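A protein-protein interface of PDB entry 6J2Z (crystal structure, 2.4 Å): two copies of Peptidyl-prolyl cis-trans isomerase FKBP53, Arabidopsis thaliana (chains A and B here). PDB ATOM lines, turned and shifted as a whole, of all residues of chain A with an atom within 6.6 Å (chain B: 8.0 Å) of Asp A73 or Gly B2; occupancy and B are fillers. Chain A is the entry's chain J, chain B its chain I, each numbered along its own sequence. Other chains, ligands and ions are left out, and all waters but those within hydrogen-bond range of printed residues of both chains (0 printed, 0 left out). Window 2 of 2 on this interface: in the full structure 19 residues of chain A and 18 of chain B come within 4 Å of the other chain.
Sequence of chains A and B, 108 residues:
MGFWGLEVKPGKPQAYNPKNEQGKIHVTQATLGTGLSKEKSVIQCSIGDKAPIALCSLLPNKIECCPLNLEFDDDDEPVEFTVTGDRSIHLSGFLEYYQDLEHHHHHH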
ATOM      1  N   PRO A  18       5.883   6.421 -15.759  1.00  0.00           N
ATOM      2  CA  PRO A  18       6.311   7.820 -15.804  1.00  0.00           C
ATOM      3  C   PRO A  18       5.190   8.873 -15.748  1.00  0.00           C
ATOM      4  O   PRO A  18       5.499   9.995 -15.435  1.00  0.00           O
ATOM      5  CB  PRO A  18       7.037   7.969 -17.156  1.00  0.00           C
ATOM      6  CG  PRO A  18       7.345   6.562 -17.608  1.00  0.00           C
ATOM      7  CD  PRO A  18       6.325   5.668 -16.937  1.00  0.00           C
ATOM      8  N   LYS A  19       3.938   8.505 -16.044  1.00  0.00           N
ATOM      9  CA  LYS A  19       2.768   9.429 -15.985  1.00  0.00           C
ATOM     10  C   LYS A  19       2.527   9.888 -14.540  1.00  0.00           C
ATOM     11  O   LYS A  19       1.873  10.930 -14.363  1.00  0.00           O
ATOM     12  CB  LYS A  19       1.503   8.765 -16.542  1.00  0.00           C
ATOM     13  CG  LYS A  19       0.367   9.705 -16.919  1.00  0.00           C
ATOM     14  CD  LYS A  19       0.748  10.707 -17.996  1.00  0.00           C
ATOM     15  CE  LYS A  19      -0.418  11.544 -18.479  1.00  0.00           C
ATOM     16  NZ  LYS A  19      -0.452  12.899 -17.868  1.00  0.00           N
ATOM     17  N   GLY A  23       6.965  15.598 -14.268  1.00  0.00           N
ATOM     18  CA  GLY A  23       7.854  16.023 -15.362  1.00  0.00           C
ATOM     19  C   GLY A  23       8.591  14.849 -15.970  1.00  0.00           C
ATOM     20  O   GLY A  23       8.342  13.707 -15.545  1.00  0.00           O
ATOM     21  N   LYS A  24       9.447  15.124 -16.955  1.00  0.00           N
ATOM     22  CA  LYS A  24      10.277  14.101 -17.642  1.00  0.00           C
ATOM     23  C   LYS A  24      11.332  13.585 -16.656  1.00  0.00           C
ATOM     24  O   LYS A  24      11.933  14.400 -15.938  1.00  0.00           O
ATOM     25  CB  LYS A  24      10.899  14.690 -18.902  1.00  0.00           C
ATOM     26  CG  LYS A  24      11.872  13.774 -19.632  1.00  0.00           C
ATOM     27  CD  LYS A  24      12.212  14.210 -21.021  1.00  0.00           C
ATOM     28  CE  LYS A  24      13.066  15.459 -21.119  1.00  0.00           C
ATOM     29  NZ  LYS A  24      13.393  15.720 -22.536  1.00  0.00           N
ATOM     30  N   ILE A  25      11.536  12.272 -16.633  1.00  0.00           N
ATOM     31  CA  ILE A  25      12.484  11.594 -15.713  1.00  0.00           C
ATOM     32  C   ILE A  25      13.835  11.452 -16.420  1.00  0.00           C
ATOM     33  O   ILE A  25      13.874  10.826 -17.489  1.00  0.00           O
ATOM     34  CB  ILE A  25      11.932  10.227 -15.286  1.00  0.00           C
ATOM     35  CG1 ILE A  25      10.529  10.373 -14.696  1.00  0.00           C
ATOM     36  CG2 ILE A  25      12.897   9.527 -14.336  1.00  0.00           C
ATOM     37  CD1 ILE A  25       9.785   9.073 -14.582  1.00  0.00           C
ATOM     38  N   GLU A  71      16.105   9.171 -20.574  1.00  0.00           N
ATOM     39  CA  GLU A  71      14.900  10.022 -20.480  1.00  0.00           C
ATOM     40  C   GLU A  71      13.660   9.141 -20.641  1.00  0.00           C
ATOM     41  O   GLU A  71      13.546   8.460 -21.676  1.00  0.00           O
ATOM     42  CB  GLU A  71      14.932  11.090 -21.567  1.00  0.00           C
ATOM     43  CG  GLU A  71      15.993  12.139 -21.311  1.00  0.00           C
ATOM     44  CD  GLU A  71      16.008  13.276 -22.303  1.00  0.00           C
ATOM     45  OE1 GLU A  71      15.026  13.400 -23.074  1.00  0.00           O
ATOM     46  OE2 GLU A  71      16.961  14.072 -22.254  1.00  0.00           O
ATOM     47  N   PHE A  72      12.786   9.157 -19.639  1.00  0.00           N
ATOM     48  CA  PHE A  72      11.440   8.534 -19.678  1.00  0.00           C
ATOM     49  C   PHE A  72      10.399   9.646 -19.582  1.00  0.00           C
ATOM     50  O   PHE A  72      10.531  10.527 -18.713  1.00  0.00           O
ATOM     51  CB  PHE A  72      11.308   7.488 -18.574  1.00  0.00           C
ATOM     52  CG  PHE A  72      12.263   6.332 -18.729  1.00  0.00           C
ATOM     53  CD1 PHE A  72      11.989   5.297 -19.609  1.00  0.00           C
ATOM     54  CD2 PHE A  72      13.462   6.308 -18.034  1.00  0.00           C
ATOM     55  CE1 PHE A  72      12.865   4.233 -19.745  1.00  0.00           C
ATOM     56  CE2 PHE A  72      14.345   5.244 -18.177  1.00  0.00           C
ATOM     57  CZ  PHE A  72      14.039   4.205 -19.029  1.00  0.00           C
ATOM     58  N   ASP A  73       9.416   9.610 -20.479  1.00  0.00           N
ATOM     59  CA  ASP A  73       8.309  10.596 -20.583  1.00  0.00           C
ATOM     60  C   ASP A  73       6.992   9.818 -20.577  1.00  0.00           C
ATOM     61  O   ASP A  73       7.036   8.578 -20.484  1.00  0.00           O
ATOM     62  CB  ASP A  73       8.487  11.488 -21.815  1.00  0.00           C
ATOM     63  CG  ASP A  73       8.621  10.752 -23.142  1.00  0.00           C
ATOM     64  OD1 ASP A  73       8.018   9.664 -23.284  1.00  0.00           O
ATOM     65  OD2 ASP A  73       9.313  11.285 -24.038  1.00  0.00           O
ATOM     66  N   ASP A  74       5.867  10.524 -20.684  1.00  0.00           N
ATOM     67  CA  ASP A  74       4.514   9.912 -20.755  1.00  0.00           C
ATOM     68  C   ASP A  74       4.481   8.833 -21.848  1.00  0.00           C
ATOM     69  O   ASP A  74       3.951   7.740 -21.561  1.00  0.00           O
ATOM     70  CB  ASP A  74       3.452  10.997 -20.905  1.00  0.00           C
ATOM     71  CG  ASP A  74       3.349  11.879 -19.669  1.00  0.00           C
ATOM     72  OD1 ASP A  74       3.939  11.517 -18.610  1.00  0.00           O
ATOM     73  OD2 ASP A  74       2.671  12.911 -19.765  1.00  0.00           O
ATOM     74  N   ASP A  75       5.071   9.094 -23.021  1.00  0.00           N
ATOM     75  CA  ASP A  75       4.932   8.231 -24.227  1.00  0.00           C
ATOM     76  C   ASP A  75       5.538   6.842 -23.987  1.00  0.00           C
ATOM     77  O   ASP A  75       5.149   5.911 -24.695  1.00  0.00           O
ATOM     78  CB  ASP A  75       5.536   8.873 -25.484  1.00  0.00           C
ATOM     79  CG  ASP A  75       5.184  10.339 -25.652  1.00  0.00           C
ATOM     80  OD1 ASP A  75       5.257  11.066 -24.646  1.00  0.00           O
ATOM     81  OD2 ASP A  75       4.791  10.733 -26.765  1.00  0.00           O
ATOM     82  N   ASP A  76       6.424   6.674 -23.006  1.00  0.00           N
ATOM     83  CA  ASP A  76       7.013   5.349 -22.660  1.00  0.00           C
ATOM     84  C   ASP A  76       5.974   4.512 -21.898  1.00  0.00           C
ATOM     85  O   ASP A  76       6.344   3.911 -20.890  1.00  0.00           O
ATOM     86  CB  ASP A  76       8.344   5.525 -21.919  1.00  0.00           C
ATOM     87  CG  ASP A  76       9.431   6.182 -22.766  1.00  0.00           C
ATOM     88  OD1 ASP A  76       9.642   5.716 -23.894  1.00  0.00           O
ATOM     89  OD2 ASP A  76      10.045   7.162 -22.304  1.00  0.00           O
ATOM     90  N   GLU A  77       4.748   4.418 -22.431  1.00  0.00           N
ATOM     91  CA  GLU A  77       3.570   3.668 -21.899  1.00  0.00           C
ATOM     92  C   GLU A  77       3.983   2.923 -20.626  1.00  0.00           C
ATOM     93  O   GLU A  77       4.560   3.547 -19.743  1.00  0.00           O
ATOM     94  CB  GLU A  77       2.949   2.874 -23.075  1.00  0.00           C
ATOM     95  CG  GLU A  77       3.774   1.706 -23.646  1.00  0.00           C
ATOM     96  CD  GLU A  77       4.790   2.038 -24.726  1.00  0.00           C
ATOM     97  OE1 GLU A  77       5.323   3.156 -24.710  1.00  0.00           O
ATOM     98  OE2 GLU A  77       5.064   1.164 -25.570  1.00  0.00           O
ATOM     99  N   VAL A  79       6.730   0.996 -18.686  1.00  0.00           N
ATOM    100  CA  VAL A  79       8.161   0.594 -18.644  1.00  0.00           C
ATOM    101  C   VAL A  79       8.276  -0.590 -17.681  1.00  0.00           C
ATOM    102  O   VAL A  79       7.728  -0.503 -16.580  1.00  0.00           O
ATOM    103  CB  VAL A  79       9.058   1.763 -18.210  1.00  0.00           C
ATOM    104  CG1 VAL A  79       9.032   2.869 -19.251  1.00  0.00           C
ATOM    105  CG2 VAL A  79       8.690   2.320 -16.861  1.00  0.00           C
ATOM    106  N   GLY B   2      11.452   9.676 -24.007  1.00  0.00           N
ATOM    107  CA  GLY B   2      11.440   8.839 -25.234  1.00  0.00           C
ATOM    108  C   GLY B   2      12.597   7.864 -25.186  1.00  0.00           C
ATOM    109  O   GLY B   2      13.676   8.201 -25.708  1.00  0.00           O
ATOM    110  N   PHE B   3      12.397   6.713 -24.543  1.00  0.00           N
ATOM    111  CA  PHE B   3      13.439   5.669 -24.412  1.00  0.00           C
ATOM    112  C   PHE B   3      13.758   5.123 -25.802  1.00  0.00           C
ATOM    113  O   PHE B   3      12.849   4.980 -26.611  1.00  0.00           O
ATOM    114  CB  PHE B   3      13.022   4.535 -23.479  1.00  0.00           C
ATOM    115  CG  PHE B   3      14.047   3.430 -23.418  1.00  0.00           C
ATOM    116  CD1 PHE B   3      15.206   3.578 -22.673  1.00  0.00           C
ATOM    117  CD2 PHE B   3      13.873   2.255 -24.133  1.00  0.00           C
ATOM    118  CE1 PHE B   3      16.157   2.568 -22.628  1.00  0.00           C
ATOM    119  CE2 PHE B   3      14.826   1.246 -24.088  1.00  0.00           C
ATOM    120  CZ  PHE B   3      15.968   1.405 -23.338  1.00  0.00           C
ATOM    121  N   TRP B   4      15.034   4.839 -26.040  1.00  0.00           N
ATOM    122  CA  TRP B   4      15.562   4.211 -27.273  1.00  0.00           C
ATOM    123  C   TRP B   4      16.580   3.139 -26.880  1.00  0.00           C
ATOM    124  O   TRP B   4      17.427   3.407 -25.977  1.00  0.00           O
ATOM    125  CB  TRP B   4      16.203   5.272 -28.171  1.00  0.00           C
ATOM    126  CG  TRP B   4      16.825   4.705 -29.407  1.00  0.00           C
ATOM    127  CD1 TRP B   4      16.235   4.560 -30.630  1.00  0.00           C
ATOM    128  CD2 TRP B   4      18.153   4.177 -29.541  1.00  0.00           C
ATOM    129  NE1 TRP B   4      17.112   4.003 -31.516  1.00  0.00           N
ATOM    130  CE2 TRP B   4      18.292   3.745 -30.874  1.00  0.00           C
ATOM    131  CE3 TRP B   4      19.236   4.034 -28.671  1.00  0.00           C
ATOM    132  CZ2 TRP B   4      19.470   3.175 -31.358  1.00  0.00           C
ATOM    133  CZ3 TRP B   4      20.398   3.466 -29.144  1.00  0.00           C
ATOM    134  CH2 TRP B   4      20.513   3.046 -30.470  1.00  0.00           C
ATOM    135  N   GLY B   5      16.528   1.995 -27.565  1.00  0.00           N
ATOM    136  CA  GLY B   5      17.454   0.875 -27.336  1.00  0.00           C
ATOM    137  C   GLY B   5      17.616   0.027 -28.577  1.00  0.00           C
ATOM    138  O   GLY B   5      16.663  -0.062 -29.352  1.00  0.00           O
ATOM    139  N   LYS B  24      15.886  12.849 -33.302  1.00  0.00           N
ATOM    140  CA  LYS B  24      17.346  12.626 -33.216  1.00  0.00           C
ATOM    141  C   LYS B  24      17.621  11.586 -32.125  1.00  0.00           C
ATOM    142  O   LYS B  24      16.998  11.659 -31.045  1.00  0.00           O
ATOM    143  CB  LYS B  24      18.065  13.948 -32.925  1.00  0.00           C
ATOM    144  CG  LYS B  24      19.567  13.819 -32.770  1.00  0.00           C
ATOM    145  CD  LYS B  24      20.193  15.020 -32.136  1.00  0.00           C
ATOM    146  CE  LYS B  24      20.441  16.145 -33.102  1.00  0.00           C
ATOM    147  NZ  LYS B  24      21.100  17.269 -32.398  1.00  0.00           N
ATOM    148  N   ILE B  25      18.512  10.642 -32.410  1.00  0.00           N
ATOM    149  CA  ILE B  25      18.876   9.542 -31.476  1.00  0.00           C
ATOM    150  C   ILE B  25      20.093   9.965 -30.656  1.00  0.00           C
ATOM    151  O   ILE B  25      21.123  10.270 -31.266  1.00  0.00           O
ATOM    152  CB  ILE B  25      19.147   8.248 -32.255  1.00  0.00           C
ATOM    153  CG1 ILE B  25      17.964   7.907 -33.164  1.00  0.00           C
ATOM    154  CG2 ILE B  25      19.488   7.115 -31.288  1.00  0.00           C
ATOM    155  CD1 ILE B  25      18.275   6.866 -34.182  1.00  0.00           C
ATOM    156  N   HIS B  26      19.933  10.005 -29.330  1.00  0.00           N
ATOM    157  CA  HIS B  26      21.015  10.158 -28.332  1.00  0.00           C
ATOM    158  C   HIS B  26      21.379   8.765 -27.811  1.00  0.00           C
ATOM    159  O   HIS B  26      20.535   8.159 -27.130  1.00  0.00           O
ATOM    160  CB  HIS B  26      20.589  11.096 -27.214  1.00  0.00           C
ATOM    161  CG  HIS B  26      20.459  12.518 -27.628  1.00  0.00           C
ATOM    162  ND1 HIS B  26      21.467  13.433 -27.442  1.00  0.00           N
ATOM    163  CD2 HIS B  26      19.422  13.196 -28.181  1.00  0.00           C
ATOM    164  CE1 HIS B  26      21.073  14.616 -27.888  1.00  0.00           C
ATOM    165  NE2 HIS B  26      19.817  14.500 -28.348  1.00  0.00           N
ATOM    166  N   GLY B  93      19.560   4.840 -24.792  1.00  0.00           N
ATOM    167  CA  GLY B  93      19.551   6.313 -24.821  1.00  0.00           C
ATOM    168  C   GLY B  93      18.132   6.834 -24.930  1.00  0.00           C
ATOM    169  O   GLY B  93      17.230   6.213 -24.340  1.00  0.00           O
ATOM    170  N   PHE B  94      17.938   7.927 -25.659  1.00  0.00           N
ATOM    171  CA  PHE B  94      16.621   8.588 -25.801  1.00  0.00           C
ATOM    172  C   PHE B  94      16.531   9.314 -27.142  1.00  0.00           C
ATOM    173  O   PHE B  94      17.578   9.556 -27.789  1.00  0.00           O
ATOM    174  CB  PHE B  94      16.393   9.533 -24.622  1.00  0.00           C
ATOM    175  CG  PHE B  94      17.412  10.634 -24.490  1.00  0.00           C
ATOM    176  CD1 PHE B  94      18.578  10.452 -23.752  1.00  0.00           C
ATOM    177  CD2 PHE B  94      17.199  11.862 -25.092  1.00  0.00           C
ATOM    178  CE1 PHE B  94      19.510  11.474 -23.629  1.00  0.00           C
ATOM    179  CE2 PHE B  94      18.132  12.886 -24.955  1.00  0.00           C
ATOM    180  CZ  PHE B  94      19.290  12.689 -24.233  1.00  0.00           C
ATOM    181  N   LEU B  95      15.298   9.659 -27.523  1.00  0.00           N
ATOM    182  CA  LEU B  95      14.961  10.461 -28.724  1.00  0.00           C
ATOM    183  C   LEU B  95      14.778  11.916 -28.302  1.00  0.00           C
ATOM    184  O   LEU B  95      14.176  12.146 -27.235  1.00  0.00           O
ATOM    185  CB  LEU B  95      13.662   9.944 -29.335  1.00  0.00           C
ATOM    186  CG  LEU B  95      13.676   8.500 -29.822  1.00  0.00           C
ATOM    187  CD1 LEU B  95      12.381   8.175 -30.561  1.00  0.00           C
ATOM    188  CD2 LEU B  95      14.862   8.226 -30.736  1.00  0.00           C
ATOM    189  N   GLU B  96      15.302  12.842 -29.105  1.00  0.00           N
ATOM    190  CA  GLU B  96      15.023  14.295 -29.007  1.00  0.00           C
ATOM    191  C   GLU B  96      14.056  14.675 -30.144  1.00  0.00           C
ATOM    192  O   GLU B  96      14.446  14.524 -31.319  1.00  0.00           O
ATOM    193  CB  GLU B  96      16.352  15.050 -29.074  1.00  0.00           C
ATOM    194  CG  GLU B  96      16.232  16.555 -28.949  1.00  0.00           C
ATOM    195  CD  GLU B  96      17.551  17.299 -29.087  1.00  0.00           C
ATOM    196  OE1 GLU B  96      18.602  16.652 -29.299  1.00  0.00           O
ATOM    197  OE2 GLU B  96      17.520  18.537 -29.004  1.00  0.00           O
ATOM    198  N   TYR B  97      12.827  15.102 -29.810  1.00  0.00           N
ATOM    199  CA  TYR B  97      11.778  15.530 -30.773  1.00  0.00           C
ATOM    200  C   TYR B  97      11.858  17.044 -30.982  1.00  0.00           C
ATOM    201  O   TYR B  97      12.575  17.481 -31.878  1.00  0.00           O
ATOM    202  CB  TYR B  97      10.379  15.159 -30.278  1.00  0.00           C
ATOM    203  CG  TYR B  97      10.230  13.735 -29.807  1.00  0.00           C
ATOM    204  CD1 TYR B  97      10.160  12.680 -30.701  1.00  0.00           C
ATOM    205  CD2 TYR B  97      10.162  13.441 -28.455  1.00  0.00           C
ATOM    206  CE1 TYR B  97      10.017  11.371 -30.269  1.00  0.00           C
ATOM    207  CE2 TYR B  97      10.022  12.138 -28.001  1.00  0.00           C
ATOM    208  CZ  TYR B  97       9.937  11.101 -28.914  1.00  0.00           C
ATOM    209  OH  TYR B  97       9.805   9.817 -28.471  1.00  0.00           O
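Of chain A, only Glu A71 (3.4 Å), Asp A73 (2.7 Å) and Asp A76 (3.3 Å) come within 4 Å of Gly B2.
Of the printed residues of chain B, Asp A76 touches Gly B2 and Phe B3.
Printed residues of chain A within 4 Å of Phe B3: Glu A71 (3.5 Å), Phe A72 (3.7 Å) and Asp A76 (3.0 Å).
Of the printed residues of chain B, Glu A71 touches Gly B2, Phe B3 and Phe B94.
Of the printed residues of chain A, Phe B94 touches Glu A71.
Gly A23 touches none of the printed residues of chain B.
Ile A25 touches none of the printed residues of chain B.
The nearest residue of chain A that does not touch Gly B2 is Phe A72 (4.5 Å).
The nearest printed residue of chain A that does not touch Phe B3 is Asp A73 (5.4 Å).
The backbone carbonyl oxygen (O) of Glu A71 lies within hydrogen-bond range of the backbone NH (N) of Gly B2, 3.4 Å away.
N of Gly B2 is in hydrogen-bond range of OD2 of Asp A73 (2.7 Å).
The backbone NH (N) of Gly B2 is in hydrogen-bond range of the side-chain carboxylate (OD2) of Asp A76, 3.3 Å away.
OD1 of Asp A76 is in hydrogen-bond range of N of Phe B3, 3.0 Å away.
Positions printed for both chains: 24 and 25.
Of the 7 pairs that touch across the chains among the printed residues, none has its exchanged pair printed and touching as well.
Among the printed residues, pairs that only touch across the chains: Glu A71 with Phe B3 (3.5 Å), Glu A71 with Phe B94 (3.2 Å) and Phe A72 with Phe B3 (3.7 Å).
The backbone carbonyl oxygen (O) of Gly B2 is in hydrogen-bond range of the backbone NH (N) of Leu B95 (2.8 Å).
N of His B26 is in hydrogen-bond range of O of Phe B94, 2.8 Å away.
OE1 of Glu A71 lies within salt-bridge range of NZ of Lys A24, at 2.9 Å.
O of Phe A72 lies within hydrogen-bond range of N of Ile A25, at 2.9 Å.
N of Asp A75 lies within hydrogen-bond range of OD1 of Asp A73 (3.0 Å).
N of Asp A73 sits at hydrogen-bond distance from OD2 of Asp A76 (3.1 Å).
Of the 13 printed residues of chain A, 4 touch a printed residue of chain B.
Printed residues of chain A that touch a printed residue of chain B: Glu A71, Phe A72, Asp A73 and Asp A76.
Of the 12 printed residues of chain B, 3 touch a printed residue of chain A.
Along chain B the printed residues that touch a printed residue of chain A span positions 2 to 94.
Among the printed residues, 7 pairs touch across the chains.
Among the printed residues, no Asp or Glu carboxylate lies within 4 Å of a Lys or Arg side-chain nitrogen of the other chain.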
